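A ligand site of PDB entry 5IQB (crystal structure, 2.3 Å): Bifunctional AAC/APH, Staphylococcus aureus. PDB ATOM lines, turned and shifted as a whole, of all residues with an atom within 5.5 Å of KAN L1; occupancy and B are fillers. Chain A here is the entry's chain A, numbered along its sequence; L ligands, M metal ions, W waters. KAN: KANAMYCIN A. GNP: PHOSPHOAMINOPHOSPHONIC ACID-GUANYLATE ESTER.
Water W1 bridges O10 of KAN L1 (2.6 Å) and OH of Tyr 274 (3.0 Å).
Water W5 lies within hydrogen-bond range of O of Asn 199 (2.6 Å), OD2 of Asp 222 (2.7 Å) and O14 of KAN L1 (2.8 Å).
Water W2 lies within hydrogen-bond range of NH1 of Arg 301 (2.6 Å) and O7 of KAN L1 (3.1 Å).
Water W7 bridges an oxygen (O15) of KAN L1 (3.4 Å) and the side-chain carboxylate of Glu 277 (3.4 Å).
Water W6 bridges the side-chain hydroxyl (OH) of Tyr 234 (3.0 Å) and an oxygen (O15) of KAN L1 (3.4 Å).
The backbone carbonyl oxygen (O) of Glu 271 sits at hydrogen-bond distance from the guanidinium group (NH2) of Arg 301, 2.9 Å away.
The backbone carbonyl oxygen (O) of Asp 222 is in hydrogen-bond range of the side-chain amide nitrogen (ND2) of Asn 199 (3.0 Å).
The backbone NH (N) of Glu 241 lies close to the side-chain hydroxyl (OG) of Ser 239 (3.4 Å).
The backbone carbonyl oxygen of Asp 200 lies within hydrogen-bond range of the side-chain hydroxyl of Ser 202.
ND1 of His 205 sits at hydrogen-bond distance from O of Asp 200 (2.9 Å).
OE2 of Glu 237 sits at hydrogen-bond distance from OG of Ser 239, 2.6 Å away.
The side-chain amide oxygen (OD1) of Asn 204 sits at hydrogen-bond distance from the side-chain hydroxyl (OG) of Ser 202 (2.6 Å).
N of Glu 242 lies within hydrogen-bond range of OG of Ser 239, 3.4 Å away.
OD1 of Asn 204 touches N3 of KAN L1 (3.9 Å).
Tyr 234 touches KAN L1 (CD1 to C11, 3.7 Å).
Ser 239 touches KAN L1.
Within 4 Å of KAN L1: Asp 200, Ser 202, Asn 204, Asp 222, Tyr 234, Glu 237, Ser 239, Glu 241, Glu 242, Glu 271, Tyr 274 and Glu 277.
OE1 of Glu 271 sits at hydrogen-bond distance from O7 of KAN L1 (2.5 Å).
The side-chain carboxylate (OD2) of Asp 222 is in salt-bridge range of a nitrogen (N4) of KAN L1 (2.6 Å).
The side-chain carboxylate (OE1) of Glu 241 lies within salt-bridge range of a nitrogen (N2) of KAN L1, at 2.6 Å.
The side-chain carboxylate of Asp 200 is in salt-bridge range of a nitrogen (N3) of KAN L1 (2.6 Å).
O15 of KAN L1 is in hydrogen-bond range of OE1 of Glu 277 (2.7 Å).
The side-chain carboxylate (OE2) of Glu 237 is in salt-bridge range of a nitrogen (N2) of KAN L1, 2.8 Å away.
The side-chain hydroxyl (OG) of Ser 202 sits at hydrogen-bond distance from a nitrogen (N3) of KAN L1 (2.8 Å).
A nitrogen (N2) of KAN L1 lies within salt-bridge range of the side-chain carboxylate (OE2) of Glu 242.
The side-chain hydroxyl of Tyr 274 sits at hydrogen-bond distance from an oxygen (O5) of KAN L1, at 3.4 Å.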
ATOM      1  N   ASN A 199      29.038   5.049  27.423  1.00  0.00           N
ATOM      2  CA  ASN A 199      28.529   3.661  27.448  1.00  0.00           C
ATOM      3  C   ASN A 199      27.073   3.479  27.195  1.00  0.00           C
ATOM      4  O   ASN A 199      26.523   2.419  27.429  1.00  0.00           O
ATOM      5  CB  ASN A 199      28.950   2.974  28.751  1.00  0.00           C
ATOM      6  CG  ASN A 199      28.991   1.475  28.640  1.00  0.00           C
ATOM      7  OD1 ASN A 199      29.265   0.925  27.581  1.00  0.00           O
ATOM      8  ND2 ASN A 199      28.720   0.806  29.720  1.00  0.00           N
ATOM      9  N   ASP A 200      26.426   4.515  26.700  1.00  0.00           N
ATOM     10  CA  ASP A 200      25.019   4.395  26.202  1.00  0.00           C
ATOM     11  C   ASP A 200      24.830   5.498  25.159  1.00  0.00           C
ATOM     12  O   ASP A 200      23.840   6.246  25.152  1.00  0.00           O
ATOM     13  CB  ASP A 200      24.027   4.462  27.309  1.00  0.00           C
ATOM     14  CG  ASP A 200      22.672   3.955  26.926  1.00  0.00           C
ATOM     15  OD1 ASP A 200      22.500   3.371  25.806  1.00  0.00           O
ATOM     16  OD2 ASP A 200      21.720   4.138  27.739  1.00  0.00           O
ATOM     17  N   SER A 202      23.890   6.798  22.239  1.00  0.00           N
ATOM     18  CA  SER A 202      22.971   6.654  21.151  1.00  0.00           C
ATOM     19  C   SER A 202      22.340   7.976  20.872  1.00  0.00           C
ATOM     20  O   SER A 202      22.469   8.893  21.712  1.00  0.00           O
ATOM     21  CB  SER A 202      21.903   5.622  21.537  1.00  0.00           C
ATOM     22  OG  SER A 202      21.339   5.948  22.786  1.00  0.00           O
ATOM     23  N   ASN A 204      19.342   9.224  20.971  1.00  0.00           N
ATOM     24  CA  ASN A 204      18.330   9.730  21.903  1.00  0.00           C
ATOM     25  C   ASN A 204      18.987  10.366  23.160  1.00  0.00           C
ATOM     26  O   ASN A 204      18.300  10.888  24.040  1.00  0.00           O
ATOM     27  CB  ASN A 204      17.346   8.635  22.309  1.00  0.00           C
ATOM     28  CG  ASN A 204      17.955   7.662  23.323  1.00  0.00           C
ATOM     29  OD1 ASN A 204      19.007   7.091  23.110  1.00  0.00           O
ATOM     30  ND2 ASN A 204      17.287   7.489  24.428  1.00  0.00           N
ATOM     31  N   HIS A 205      20.320  10.374  23.224  1.00  0.00           N
ATOM     32  CA  HIS A 205      21.046  11.054  24.253  1.00  0.00           C
ATOM     33  C   HIS A 205      21.851  12.228  23.766  1.00  0.00           C
ATOM     34  O   HIS A 205      22.561  12.870  24.548  1.00  0.00           O
ATOM     35  CB  HIS A 205      21.913  10.057  25.017  1.00  0.00           C
ATOM     36  CG  HIS A 205      21.130   9.087  25.831  1.00  0.00           C
ATOM     37  ND1 HIS A 205      21.550   7.807  26.083  1.00  0.00           N
ATOM     38  CD2 HIS A 205      19.934   9.202  26.458  1.00  0.00           C
ATOM     39  CE1 HIS A 205      20.644   7.169  26.815  1.00  0.00           C
ATOM     40  NE2 HIS A 205      19.646   8.001  27.061  1.00  0.00           N
ATOM     41  N   ASP A 219      22.477  11.476  30.113  1.00  0.00           N
ATOM     42  CA  ASP A 219      22.400  10.054  30.543  1.00  0.00           C
ATOM     43  C   ASP A 219      23.744   9.361  30.512  1.00  0.00           C
ATOM     44  O   ASP A 219      24.012   8.517  29.679  1.00  0.00           O
ATOM     45  CB  ASP A 219      21.381   9.277  29.719  1.00  0.00           C
ATOM     46  CG  ASP A 219      20.982   7.978  30.383  1.00  0.00           C
ATOM     47  OD1 ASP A 219      21.663   7.642  31.392  1.00  0.00           O
ATOM     48  OD2 ASP A 219      19.955   7.311  29.978  1.00  0.00           O
ATOM     49  N   ASP A 222      25.325   4.819  32.624  1.00  0.00           N
ATOM     50  CA  ASP A 222      26.005   3.544  32.448  1.00  0.00           C
ATOM     51  C   ASP A 222      27.498   3.716  32.301  1.00  0.00           C
ATOM     52  O   ASP A 222      28.210   2.755  31.953  1.00  0.00           O
ATOM     53  CB  ASP A 222      25.466   2.840  31.190  1.00  0.00           C
ATOM     54  CG  ASP A 222      24.016   2.351  31.322  1.00  0.00           C
ATOM     55  OD1 ASP A 222      23.464   2.306  32.425  1.00  0.00           O
ATOM     56  OD2 ASP A 222      23.423   1.960  30.294  1.00  0.00           O
ATOM     57  N   TYR A 234      26.450   2.112  19.364  1.00  0.00           N
ATOM     58  CA  TYR A 234      25.193   2.578  18.865  1.00  0.00           C
ATOM     59  C   TYR A 234      25.402   3.477  17.678  1.00  0.00           C
ATOM     60  O   TYR A 234      24.562   3.530  16.778  1.00  0.00           O
ATOM     61  CB  TYR A 234      24.344   3.242  19.982  1.00  0.00           C
ATOM     62  CG  TYR A 234      24.074   2.249  21.076  1.00  0.00           C
ATOM     63  CD1 TYR A 234      23.456   1.043  20.794  1.00  0.00           C
ATOM     64  CD2 TYR A 234      24.434   2.489  22.386  1.00  0.00           C
ATOM     65  CE1 TYR A 234      23.221   0.084  21.763  1.00  0.00           C
ATOM     66  CE2 TYR A 234      24.181   1.551  23.378  1.00  0.00           C
ATOM     67  CZ  TYR A 234      23.570   0.369  23.044  1.00  0.00           C
ATOM     68  OH  TYR A 234      23.333  -0.575  23.985  1.00  0.00           O
ATOM     69  N   GLU A 237      25.332   1.165  14.952  1.00  0.00           N
ATOM     70  CA  GLU A 237      24.117   0.318  14.892  1.00  0.00           C
ATOM     71  C   GLU A 237      23.305   0.623  13.658  1.00  0.00           C
ATOM     72  O   GLU A 237      23.127   1.765  13.279  1.00  0.00           O
ATOM     73  CB  GLU A 237      23.253   0.469  16.146  1.00  0.00           C
ATOM     74  CG  GLU A 237      21.962  -0.333  16.143  1.00  0.00           C
ATOM     75  CD  GLU A 237      21.261  -0.286  17.519  1.00  0.00           C
ATOM     76  OE1 GLU A 237      21.851  -0.799  18.508  1.00  0.00           O
ATOM     77  OE2 GLU A 237      20.114   0.262  17.602  1.00  0.00           O
ATOM     78  N   SER A 239      19.687   0.230  12.648  1.00  0.00           N
ATOM     79  CA  SER A 239      18.341   0.026  13.179  1.00  0.00           C
ATOM     80  C   SER A 239      17.491   1.259  12.995  1.00  0.00           C
ATOM     81  O   SER A 239      18.000   2.309  12.600  1.00  0.00           O
ATOM     82  CB  SER A 239      18.411  -0.300  14.680  1.00  0.00           C
ATOM     83  OG  SER A 239      18.776   0.852  15.432  1.00  0.00           O
ATOM     84  N   GLU A 241      16.127   3.036  15.276  1.00  0.00           N
ATOM     85  CA  GLU A 241      16.472   4.027  16.293  1.00  0.00           C
ATOM     86  C   GLU A 241      17.727   4.834  15.983  1.00  0.00           C
ATOM     87  O   GLU A 241      17.885   5.981  16.459  1.00  0.00           O
ATOM     88  CB  GLU A 241      16.641   3.350  17.646  1.00  0.00           C
ATOM     89  CG  GLU A 241      15.368   2.735  18.199  1.00  0.00           C
ATOM     90  CD  GLU A 241      15.546   2.025  19.538  1.00  0.00           C
ATOM     91  OE1 GLU A 241      16.622   2.104  20.167  1.00  0.00           O
ATOM     92  OE2 GLU A 241      14.572   1.392  19.985  1.00  0.00           O
ATOM     93  N   GLU A 242      18.659   4.250  15.233  1.00  0.00           N
ATOM     94  CA  GLU A 242      19.962   4.884  15.052  1.00  0.00           C
ATOM     95  C   GLU A 242      20.139   5.296  13.602  1.00  0.00           C
ATOM     96  O   GLU A 242      19.370   4.914  12.747  1.00  0.00           O
ATOM     97  CB  GLU A 242      21.091   3.983  15.519  1.00  0.00           C
ATOM     98  CG  GLU A 242      20.975   3.513  16.951  1.00  0.00           C
ATOM     99  CD  GLU A 242      20.896   4.637  17.992  1.00  0.00           C
ATOM    100  OE1 GLU A 242      21.587   5.706  17.870  1.00  0.00           O
ATOM    101  OE2 GLU A 242      20.152   4.405  18.971  1.00  0.00           O
ATOM    102  N   GLU A 271      25.378  -6.609  19.993  1.00  0.00           N
ATOM    103  CA  GLU A 271      24.032  -6.806  19.422  1.00  0.00           C
ATOM    104  C   GLU A 271      23.584  -8.281  19.513  1.00  0.00           C
ATOM    105  O   GLU A 271      22.420  -8.566  19.764  1.00  0.00           O
ATOM    106  CB  GLU A 271      23.947  -6.307  18.003  1.00  0.00           C
ATOM    107  CG  GLU A 271      22.498  -6.187  17.503  1.00  0.00           C
ATOM    108  CD  GLU A 271      22.292  -4.993  16.562  1.00  0.00           C
ATOM    109  OE1 GLU A 271      21.427  -4.133  16.843  1.00  0.00           O
ATOM    110  OE2 GLU A 271      23.040  -4.893  15.551  1.00  0.00           O
ATOM    111  N   TYR A 274      22.122  -8.949  23.016  1.00  0.00           N
ATOM    112  CA  TYR A 274      20.937  -8.187  23.461  1.00  0.00           C
ATOM    113  C   TYR A 274      19.747  -8.994  23.952  1.00  0.00           C
ATOM    114  O   TYR A 274      19.236  -8.750  25.021  1.00  0.00           O
ATOM    115  CB  TYR A 274      20.500  -7.217  22.361  1.00  0.00           C
ATOM    116  CG  TYR A 274      19.271  -6.413  22.644  1.00  0.00           C
ATOM    117  CD1 TYR A 274      19.281  -5.413  23.577  1.00  0.00           C
ATOM    118  CD2 TYR A 274      18.090  -6.639  21.945  1.00  0.00           C
ATOM    119  CE1 TYR A 274      18.136  -4.670  23.802  1.00  0.00           C
ATOM    120  CE2 TYR A 274      16.950  -5.878  22.154  1.00  0.00           C
ATOM    121  CZ  TYR A 274      16.977  -4.922  23.086  1.00  0.00           C
ATOM    122  OH  TYR A 274      15.852  -4.155  23.319  1.00  0.00           O
ATOM    123  N   GLU A 277      20.755 -10.508  27.255  1.00  0.00           N
ATOM    124  CA  GLU A 277      20.774  -9.449  28.281  1.00  0.00           C
ATOM    125  C   GLU A 277      19.355  -9.117  28.737  1.00  0.00           C
ATOM    126  O   GLU A 277      19.113  -8.860  29.912  1.00  0.00           O
ATOM    127  CB  GLU A 277      21.378  -8.198  27.735  1.00  0.00           C
ATOM    128  CG  GLU A 277      21.574  -7.147  28.802  1.00  0.00           C
ATOM    129  CD  GLU A 277      22.167  -5.893  28.237  1.00  0.00           C
ATOM    130  OE1 GLU A 277      21.511  -5.316  27.354  1.00  0.00           O
ATOM    131  OE2 GLU A 277      23.294  -5.525  28.654  1.00  0.00           O
ATOM    132  N   ARG A 301      15.518 -13.525  15.543  1.00  0.00           N
ATOM    133  CA  ARG A 301      16.892 -13.508  14.993  1.00  0.00           C
ATOM    134  C   ARG A 301      17.300 -14.839  14.293  1.00  0.00           C
ATOM    135  O   ARG A 301      17.882 -14.829  13.230  1.00  0.00           O
ATOM    136  CB  ARG A 301      17.906 -13.123  16.091  1.00  0.00           C
ATOM    137  CG  ARG A 301      17.942 -11.638  16.448  1.00  0.00           C
ATOM    138  CD  ARG A 301      18.653 -11.448  17.764  1.00  0.00           C
ATOM    139  NE  ARG A 301      19.547 -10.278  17.924  1.00  0.00           N
ATOM    140  CZ  ARG A 301      19.121  -9.046  18.160  1.00  0.00           C
ATOM    141  NH1 ARG A 301      17.827  -8.772  18.177  1.00  0.00           N
ATOM    142  NH2 ARG A 301      19.985  -8.057  18.322  1.00  0.00           N
HETATM  143  C1  KAN L   1      18.893  -2.100  21.165  1.00  0.00           C
HETATM  144  C2  KAN L   1      19.417  -3.063  20.106  1.00  0.00           C
HETATM  145  C3  KAN L   1      18.770  -2.799  18.747  1.00  0.00           C
HETATM  146  C4  KAN L   1      17.260  -2.751  18.864  1.00  0.00           C
HETATM  147  C5  KAN L   1      16.870  -1.713  19.886  1.00  0.00           C
HETATM  148  C6  KAN L   1      15.368  -1.670  20.076  1.00  0.00           C
HETATM  149  C7  KAN L   1      20.361   2.453  23.355  1.00  0.00           C
HETATM  150  C8  KAN L   1      19.528   1.357  24.006  1.00  0.00           C
HETATM  151  C9  KAN L   1      19.618   0.045  23.208  1.00  0.00           C
HETATM  152  C10 KAN L   1      19.117   0.283  21.786  1.00  0.00           C
HETATM  153  C11 KAN L   1      19.809   1.471  21.111  1.00  0.00           C
HETATM  154  C12 KAN L   1      19.756   2.741  21.980  1.00  0.00           C
HETATM  155  C13 KAN L   1      19.252   0.630  26.273  1.00  0.00           C
HETATM  156  C14 KAN L   1      19.421   1.385  27.589  1.00  0.00           C
HETATM  157  C15 KAN L   1      20.810   1.136  28.183  1.00  0.00           C
HETATM  158  C16 KAN L   1      21.015  -0.362  28.300  1.00  0.00           C
HETATM  159  C17 KAN L   1      20.802  -1.081  26.979  1.00  0.00           C
HETATM  160  C18 KAN L   1      20.869  -2.586  27.144  1.00  0.00           C
HETATM  161  N1  KAN L   1      15.040  -0.909  21.277  1.00  0.00           N
HETATM  162  N2  KAN L   1      19.163   1.728  19.813  1.00  0.00           N
HETATM  163  N3  KAN L   1      20.480   3.654  24.196  1.00  0.00           N
HETATM  164  N4  KAN L   1      21.004   1.699  29.519  1.00  0.00           N
HETATM  165  O5  KAN L   1      17.472  -2.042  21.152  1.00  0.00           O
HETATM  166  O6  KAN L   1      20.827  -2.881  19.994  1.00  0.00           O
HETATM  167  O7  KAN L   1      19.107  -3.812  17.823  1.00  0.00           O
HETATM  168  O8  KAN L   1      16.710  -2.379  17.632  1.00  0.00           O
HETATM  169  O9  KAN L   1      19.497  -0.824  20.958  1.00  0.00           O
HETATM  170  O10 KAN L   1      18.808  -0.950  23.830  1.00  0.00           O
HETATM  171  O11 KAN L   1      20.126   1.142  25.291  1.00  0.00           O
HETATM  172  O12 KAN L   1      19.504  -0.752  26.453  1.00  0.00           O
HETATM  173  O13 KAN L   1      19.240   2.781  27.385  1.00  0.00           O
HETATM  174  O14 KAN L   1      22.349  -0.584  28.701  1.00  0.00           O
HETATM  175  O15 KAN L   1      20.520  -3.274  25.939  1.00  0.00           O
HETATM  176  PG  GNP L   2      18.261   5.495  33.467  1.00  0.00           P
HETATM  177  O1G GNP L   2      18.073   4.135  32.983  1.00  0.00           O
HETATM  178  O2G GNP L   2      18.385   5.431  35.001  1.00  0.00           O
HETATM  179  O3G GNP L   2      19.466   6.295  32.829  1.00  0.00           O
HETATM  180  N3B GNP L   2      16.950   6.409  33.124  1.00  0.00           N
HETATM  181  PB  GNP L   2      16.663   7.111  31.687  1.00  0.00           P
HETATM  182  O1B GNP L   2      17.336   6.459  30.571  1.00  0.00           O
HETATM  183  O2B GNP L   2      15.212   7.072  31.363  1.00  0.00           O
HETATM  184  O3A GNP L   2      17.143   8.610  31.931  1.00  0.00           O
HETATM  185  PA  GNP L   2      17.688   9.720  30.922  1.00  0.00           P
HETATM  186  O1A GNP L   2      18.012   9.221  29.543  1.00  0.00           O
HETATM  187  O2A GNP L   2      18.902  10.184  31.648  1.00  0.00           O
HETATM  188  O5' GNP L   2      16.603  10.885  30.856  1.00  0.00           O
HETATM  189  C5' GNP L   2      15.245  10.486  30.649  1.00  0.00           C
HETATM  190  C4' GNP L   2      14.734  11.353  29.535  1.00  0.00           C
HETATM  191  O4' GNP L   2      14.529  12.693  30.023  1.00  0.00           O
HETATM  192  C3' GNP L   2      15.640  11.533  28.333  1.00  0.00           C
HETATM  193  O3' GNP L   2      15.393  10.520  27.386  1.00  0.00           O
HETATM  194  C2' GNP L   2      15.147  12.852  27.758  1.00  0.00           C
HETATM  195  O2' GNP L   2      13.896  12.717  27.093  1.00  0.00           O
HETATM  196  C1' GNP L   2      14.859  13.639  29.038  1.00  0.00           C
HETATM  197  N9  GNP L   2      15.996  14.441  29.504  1.00  0.00           N
HETATM  198  C8  GNP L   2      16.881  14.143  30.508  1.00  0.00           C
HETATM  199  N7  GNP L   2      17.815  15.060  30.650  1.00  0.00           N
HETATM  200  C5  GNP L   2      17.484  16.023  29.706  1.00  0.00           C
HETATM  201  C6  GNP L   2      18.064  17.232  29.461  1.00  0.00           C
HETATM  202  O6  GNP L   2      18.989  17.737  30.090  1.00  0.00           O
HETATM  203  N1  GNP L   2      17.488  17.887  28.396  1.00  0.00           N
HETATM  204  C2  GNP L   2      16.412  17.441  27.697  1.00  0.00           C
HETATM  205  N2  GNP L   2      15.985  18.170  26.681  1.00  0.00           N
HETATM  206  N3  GNP L   2      15.801  16.296  27.990  1.00  0.00           N
HETATM  207  C4  GNP L   2      16.397  15.639  28.991  1.00  0.00           C
HETATM  208 MG    MG M   1      20.517   5.790  31.398  1.00  0.00          MG
HETATM  209 MG    MG M   2      18.300   7.408  28.706  1.00  0.00          MG
HETATM  210  O   HOH W   1      16.254  -1.211  23.840  1.00  0.00           O
HETATM  211  O   HOH W   2      17.377  -6.341  17.360  1.00  0.00           O
HETATM  212  O   HOH W   3      17.310  -3.417  15.173  1.00  0.00           O
HETATM  213  O   HOH W   4      18.411   5.229  28.206  1.00  0.00           O
HETATM  214  O   HOH W   5      24.823   0.693  28.371  1.00  0.00           O
HETATM  215  O   HOH W   6      22.362  -3.281  23.049  1.00  0.00           O
HETATM  216  O   HOH W   7      18.083  -5.349  26.997  1.00  0.00           O
